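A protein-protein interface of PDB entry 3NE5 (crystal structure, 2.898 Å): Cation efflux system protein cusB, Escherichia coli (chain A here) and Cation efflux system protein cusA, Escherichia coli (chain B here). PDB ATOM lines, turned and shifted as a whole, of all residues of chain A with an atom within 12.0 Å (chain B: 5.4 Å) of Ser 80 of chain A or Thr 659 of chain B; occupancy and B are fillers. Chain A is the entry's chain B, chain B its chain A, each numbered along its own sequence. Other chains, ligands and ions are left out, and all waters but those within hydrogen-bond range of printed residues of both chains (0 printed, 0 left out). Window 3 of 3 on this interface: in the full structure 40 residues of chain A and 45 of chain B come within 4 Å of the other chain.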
ATOM      1  N   ALA A  79     -19.916  15.207 -10.338  1.00  0.00           N
ATOM      2  CA  ALA A  79     -21.086  14.746 -11.076  1.00  0.00           C
ATOM      3  C   ALA A  79     -21.690  15.873 -11.907  1.00  0.00           C
ATOM      4  O   ALA A  79     -22.900  16.096 -11.880  1.00  0.00           O
ATOM      5  CB  ALA A  79     -22.123  14.173 -10.122  1.00  0.00           C
ATOM      6  N   SER A  80     -20.840  16.579 -12.646  1.00  0.00           N
ATOM      7  CA  SER A  80     -21.287  17.696 -13.470  1.00  0.00           C
ATOM      8  C   SER A  80     -22.100  17.227 -14.672  1.00  0.00           C
ATOM      9  O   SER A  80     -21.653  16.377 -15.443  1.00  0.00           O
ATOM     10  CB  SER A  80     -20.093  18.527 -13.945  1.00  0.00           C
ATOM     11  OG  SER A  80     -19.464  19.188 -12.862  1.00  0.00           O
ATOM     12  N   GLY A  81     -23.295  17.787 -14.824  1.00  0.00           N
ATOM     13  CA  GLY A  81     -24.127  17.507 -15.980  1.00  0.00           C
ATOM     14  C   GLY A  81     -23.827  18.481 -17.103  1.00  0.00           C
ATOM     15  O   GLY A  81     -24.647  18.688 -17.998  1.00  0.00           O
ATOM     16  N   VAL A  82     -22.642  19.081 -17.047  1.00  0.00           N
ATOM     17  CA  VAL A  82     -22.217  20.057 -18.043  1.00  0.00           C
ATOM     18  C   VAL A  82     -22.044  19.405 -19.412  1.00  0.00           C
ATOM     19  O   VAL A  82     -21.210  18.517 -19.589  1.00  0.00           O
ATOM     20  CB  VAL A  82     -20.904  20.750 -17.621  1.00  0.00           C
ATOM     21  CG1 VAL A  82     -19.823  19.716 -17.337  1.00  0.00           C
ATOM     22  CG2 VAL A  82     -20.452  21.736 -18.687  1.00  0.00           C
ATOM     23  N   ARG A  83     -22.841  19.852 -20.377  1.00  0.00           N
ATOM     24  CA  ARG A  83     -22.840  19.252 -21.705  1.00  0.00           C
ATOM     25  C   ARG A  83     -22.010  20.045 -22.703  1.00  0.00           C
ATOM     26  O   ARG A  83     -21.858  21.261 -22.584  1.00  0.00           O
ATOM     27  CB  ARG A  83     -24.269  19.100 -22.228  1.00  0.00           C
ATOM     28  CG  ARG A  83     -25.048  17.968 -21.588  1.00  0.00           C
ATOM     29  CD  ARG A  83     -24.395  16.627 -21.873  1.00  0.00           C
ATOM     30  NE  ARG A  83     -24.009  16.496 -23.275  1.00  0.00           N
ATOM     31  CZ  ARG A  83     -24.846  16.172 -24.256  1.00  0.00           C
ATOM     32  NH1 ARG A  83     -26.126  15.945 -23.992  1.00  0.00           N
ATOM     33  NH2 ARG A  83     -24.403  16.076 -25.502  1.00  0.00           N
ATOM     34  N   ILE A  84     -21.480  19.341 -23.694  1.00  0.00           N
ATOM     35  CA  ILE A  84     -20.675  19.960 -24.733  1.00  0.00           C
ATOM     36  C   ILE A  84     -21.062  19.390 -26.090  1.00  0.00           C
ATOM     37  O   ILE A  84     -21.531  18.254 -26.185  1.00  0.00           O
ATOM     38  CB  ILE A  84     -19.181  19.707 -24.484  1.00  0.00           C
ATOM     39  CG1 ILE A  84     -18.369  19.939 -25.755  1.00  0.00           C
ATOM     40  CG2 ILE A  84     -18.963  18.288 -24.012  1.00  0.00           C
ATOM     41  CD1 ILE A  84     -17.098  19.121 -25.805  1.00  0.00           C
ATOM     42  N   ASP A  85     -20.883  20.186 -27.137  1.00  0.00           N
ATOM     43  CA  ASP A  85     -21.112  19.718 -28.494  1.00  0.00           C
ATOM     44  C   ASP A  85     -19.928  18.878 -28.960  1.00  0.00           C
ATOM     45  O   ASP A  85     -18.832  19.400 -29.161  1.00  0.00           O
ATOM     46  CB  ASP A  85     -21.313  20.899 -29.438  1.00  0.00           C
ATOM     47  CG  ASP A  85     -21.455  20.467 -30.876  1.00  0.00           C
ATOM     48  OD1 ASP A  85     -21.978  19.358 -31.111  1.00  0.00           O
ATOM     49  OD2 ASP A  85     -21.045  21.235 -31.771  1.00  0.00           O
ATOM     50  N   LEU B 602     -14.717  21.690 -22.788  1.00  0.00           N
ATOM     51  CA  LEU B 602     -15.108  21.534 -21.391  1.00  0.00           C
ATOM     52  C   LEU B 602     -14.278  22.416 -20.461  1.00  0.00           C
ATOM     53  O   LEU B 602     -14.801  22.987 -19.505  1.00  0.00           O
ATOM     54  CB  LEU B 602     -14.997  20.070 -20.969  1.00  0.00           C
ATOM     55  CG  LEU B 602     -16.032  19.148 -21.614  1.00  0.00           C
ATOM     56  CD1 LEU B 602     -15.808  17.698 -21.209  1.00  0.00           C
ATOM     57  CD2 LEU B 602     -17.431  19.608 -21.241  1.00  0.00           C
ATOM     58  N   SER B 605     -15.344  25.899 -20.712  1.00  0.00           N
ATOM     59  CA  SER B 605     -16.693  26.104 -20.189  1.00  0.00           C
ATOM     60  C   SER B 605     -16.660  26.534 -18.726  1.00  0.00           C
ATOM     61  O   SER B 605     -17.699  26.807 -18.123  1.00  0.00           O
ATOM     62  CB  SER B 605     -17.536  24.837 -20.344  1.00  0.00           C
ATOM     63  OG  SER B 605     -17.181  23.866 -19.377  1.00  0.00           O
ATOM     64  N   VAL B 606     -15.458  26.584 -18.160  1.00  0.00           N
ATOM     65  CA  VAL B 606     -15.263  27.073 -16.802  1.00  0.00           C
ATOM     66  C   VAL B 606     -14.934  28.562 -16.844  1.00  0.00           C
ATOM     67  O   VAL B 606     -14.065  28.989 -17.602  1.00  0.00           O
ATOM     68  CB  VAL B 606     -14.148  26.303 -16.078  1.00  0.00           C
ATOM     69  CG1 VAL B 606     -13.838  26.949 -14.737  1.00  0.00           C
ATOM     70  CG2 VAL B 606     -14.555  24.850 -15.892  1.00  0.00           C
ATOM     71  N   GLU B 654     -10.766  21.702  -9.015  1.00  0.00           N
ATOM     72  CA  GLU B 654     -11.779  20.714  -8.674  1.00  0.00           C
ATOM     73  C   GLU B 654     -12.930  20.758  -9.672  1.00  0.00           C
ATOM     74  O   GLU B 654     -13.464  19.721 -10.063  1.00  0.00           O
ATOM     75  CB  GLU B 654     -12.295  20.932  -7.251  1.00  0.00           C
ATOM     76  CG  GLU B 654     -12.637  19.641  -6.527  1.00  0.00           C
ATOM     77  CD  GLU B 654     -11.427  18.740  -6.357  1.00  0.00           C
ATOM     78  OE1 GLU B 654     -11.604  17.504  -6.306  1.00  0.00           O
ATOM     79  OE2 GLU B 654     -10.296  19.268  -6.280  1.00  0.00           O
ATOM     80  N   GLU B 655     -13.305  21.966 -10.082  1.00  0.00           N
ATOM     81  CA  GLU B 655     -14.348  22.133 -11.084  1.00  0.00           C
ATOM     82  C   GLU B 655     -13.856  21.620 -12.437  1.00  0.00           C
ATOM     83  O   GLU B 655     -14.621  21.046 -13.209  1.00  0.00           O
ATOM     84  CB  GLU B 655     -14.778  23.600 -11.185  1.00  0.00           C
ATOM     85  CG  GLU B 655     -16.006  23.828 -12.055  1.00  0.00           C
ATOM     86  CD  GLU B 655     -16.558  25.235 -11.934  1.00  0.00           C
ATOM     87  OE1 GLU B 655     -16.927  25.823 -12.971  1.00  0.00           O
ATOM     88  OE2 GLU B 655     -16.625  25.757 -10.800  1.00  0.00           O
ATOM     89  N   LEU B 656     -12.571  21.827 -12.716  1.00  0.00           N
ATOM     90  CA  LEU B 656     -11.956  21.303 -13.933  1.00  0.00           C
ATOM     91  C   LEU B 656     -11.959  19.780 -13.937  1.00  0.00           C
ATOM     92  O   LEU B 656     -12.418  19.157 -14.895  1.00  0.00           O
ATOM     93  CB  LEU B 656     -10.524  21.820 -14.081  1.00  0.00           C
ATOM     94  CG  LEU B 656     -10.257  22.896 -15.137  1.00  0.00           C
ATOM     95  CD1 LEU B 656     -11.425  23.856 -15.247  1.00  0.00           C
ATOM     96  CD2 LEU B 656      -8.976  23.651 -14.809  1.00  0.00           C
ATOM     97  N   ASP B 657     -11.446  19.184 -12.867  1.00  0.00           N
ATOM     98  CA  ASP B 657     -11.345  17.733 -12.784  1.00  0.00           C
ATOM     99  C   ASP B 657     -12.717  17.076 -12.720  1.00  0.00           C
ATOM    100  O   ASP B 657     -12.866  15.899 -13.044  1.00  0.00           O
ATOM    101  CB  ASP B 657     -10.523  17.316 -11.565  1.00  0.00           C
ATOM    102  CG  ASP B 657     -10.184  15.840 -11.573  1.00  0.00           C
ATOM    103  OD1 ASP B 657     -10.768  15.088 -10.764  1.00  0.00           O
ATOM    104  OD2 ASP B 657      -9.343  15.428 -12.398  1.00  0.00           O
ATOM    105  N   ASN B 658     -13.720  17.835 -12.296  1.00  0.00           N
ATOM    106  CA  ASN B 658     -15.064  17.292 -12.159  1.00  0.00           C
ATOM    107  C   ASN B 658     -15.902  17.550 -13.403  1.00  0.00           C
ATOM    108  O   ASN B 658     -16.870  16.838 -13.671  1.00  0.00           O
ATOM    109  CB  ASN B 658     -15.756  17.872 -10.926  1.00  0.00           C
ATOM    110  CG  ASN B 658     -16.884  16.994 -10.428  1.00  0.00           C
ATOM    111  OD1 ASN B 658     -18.019  17.445 -10.280  1.00  0.00           O
ATOM    112  ND2 ASN B 658     -16.576  15.728 -10.171  1.00  0.00           N
ATOM    113  N   THR B 659     -15.519  18.575 -14.156  1.00  0.00           N
ATOM    114  CA  THR B 659     -16.212  18.944 -15.384  1.00  0.00           C
ATOM    115  C   THR B 659     -15.589  18.261 -16.596  1.00  0.00           C
ATOM    116  O   THR B 659     -16.286  17.657 -17.409  1.00  0.00           O
ATOM    117  CB  THR B 659     -16.179  20.469 -15.607  1.00  0.00           C
ATOM    118  OG1 THR B 659     -17.077  21.110 -14.692  1.00  0.00           O
ATOM    119  CG2 THR B 659     -16.582  20.811 -17.032  1.00  0.00           C
ATOM    120  N   VAL B 660     -14.268  18.360 -16.705  1.00  0.00           N
ATOM    121  CA  VAL B 660     -13.542  17.797 -17.836  1.00  0.00           C
ATOM    122  C   VAL B 660     -13.123  16.359 -17.576  1.00  0.00           C
ATOM    123  O   VAL B 660     -12.032  16.105 -17.071  1.00  0.00           O
ATOM    124  CB  VAL B 660     -12.277  18.615 -18.150  1.00  0.00           C
ATOM    125  CG1 VAL B 660     -11.551  18.022 -19.346  1.00  0.00           C
ATOM    126  CG2 VAL B 660     -12.632  20.068 -18.406  1.00  0.00           C
ATOM    127  N   ARG B 661     -13.990  15.418 -17.928  1.00  0.00           N
ATOM    128  CA  ARG B 661     -13.660  14.007 -17.784  1.00  0.00           C
ATOM    129  C   ARG B 661     -14.372  13.138 -18.818  1.00  0.00           C
ATOM    130  O   ARG B 661     -15.581  13.253 -19.024  1.00  0.00           O
ATOM    131  CB  ARG B 661     -13.946  13.520 -16.357  1.00  0.00           C
ATOM    132  CG  ARG B 661     -15.332  13.857 -15.843  1.00  0.00           C
ATOM    133  CD  ARG B 661     -15.400  13.787 -14.320  1.00  0.00           C
ATOM    134  NE  ARG B 661     -15.031  12.474 -13.796  1.00  0.00           N
ATOM    135  CZ  ARG B 661     -13.934  12.231 -13.086  1.00  0.00           C
ATOM    136  NH1 ARG B 661     -13.680  11.006 -12.648  1.00  0.00           N
ATOM    137  NH2 ARG B 661     -13.090  13.216 -12.808  1.00  0.00           N
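The backbone NH of Ala 79 of chain A is in hydrogen-bond range of the side-chain amide oxygen of Asn 658 of chain B, at 2.9 Å.
OD1 of Asn 658 of chain B is in hydrogen-bond range of OG of Ser 80 of chain A, 3.4 Å away.
O of Leu 602 of chain B lies within hydrogen-bond range of OG of Ser 605 of chain B, at 2.5 Å.
O of Glu 655 of chain B sits at hydrogen-bond distance from OG1 of Thr 659 of chain B (2.9 Å).
Among the printed residues, merely in contact across the chains: Ser 80 of chain A with Thr 659 of chain B, Val 82 of chain A with Ser 605 of chain B, Val 82 of chain A with Thr 659 of chain B and Ile 84 of chain A with Leu 602 of chain B.
Of chain B, only Asn 658 and Thr 659 come within 4 Å of Ser 80 of chain A.
Thr 659 of chain B touches two residues of chain A.
Leu 602 of chain B touches just one residue of chain A: Ile 84.
Ser 605 of chain B touches just one residue of chain A: Val 82.
Asn 658 of chain B touches just these residues of chain A: Ala 79 and Ser 80.
No residue of chain A comes within 4 Å of Arg 661 of chain B.
Of the printed residues of chain B, Ala 79 of chain A touches Asn 658.
Of the printed residues of chain B, Val 82 of chain A touches Ser 605 (3.96 Å) and Thr 659 (3.4 Å).
Arg 83 of chain A touches none of the printed residues of chain B.
Of the 7 printed residues of chain A, 4 touch a printed residue of chain B.
Hydrophobic or aromatic side chains of chain B that line the printed part of chain A: Leu 602.
Among the printed residues, no Asp or Glu carboxylate lies within 4 Å of a Lys or Arg side-chain nitrogen of the other chain.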
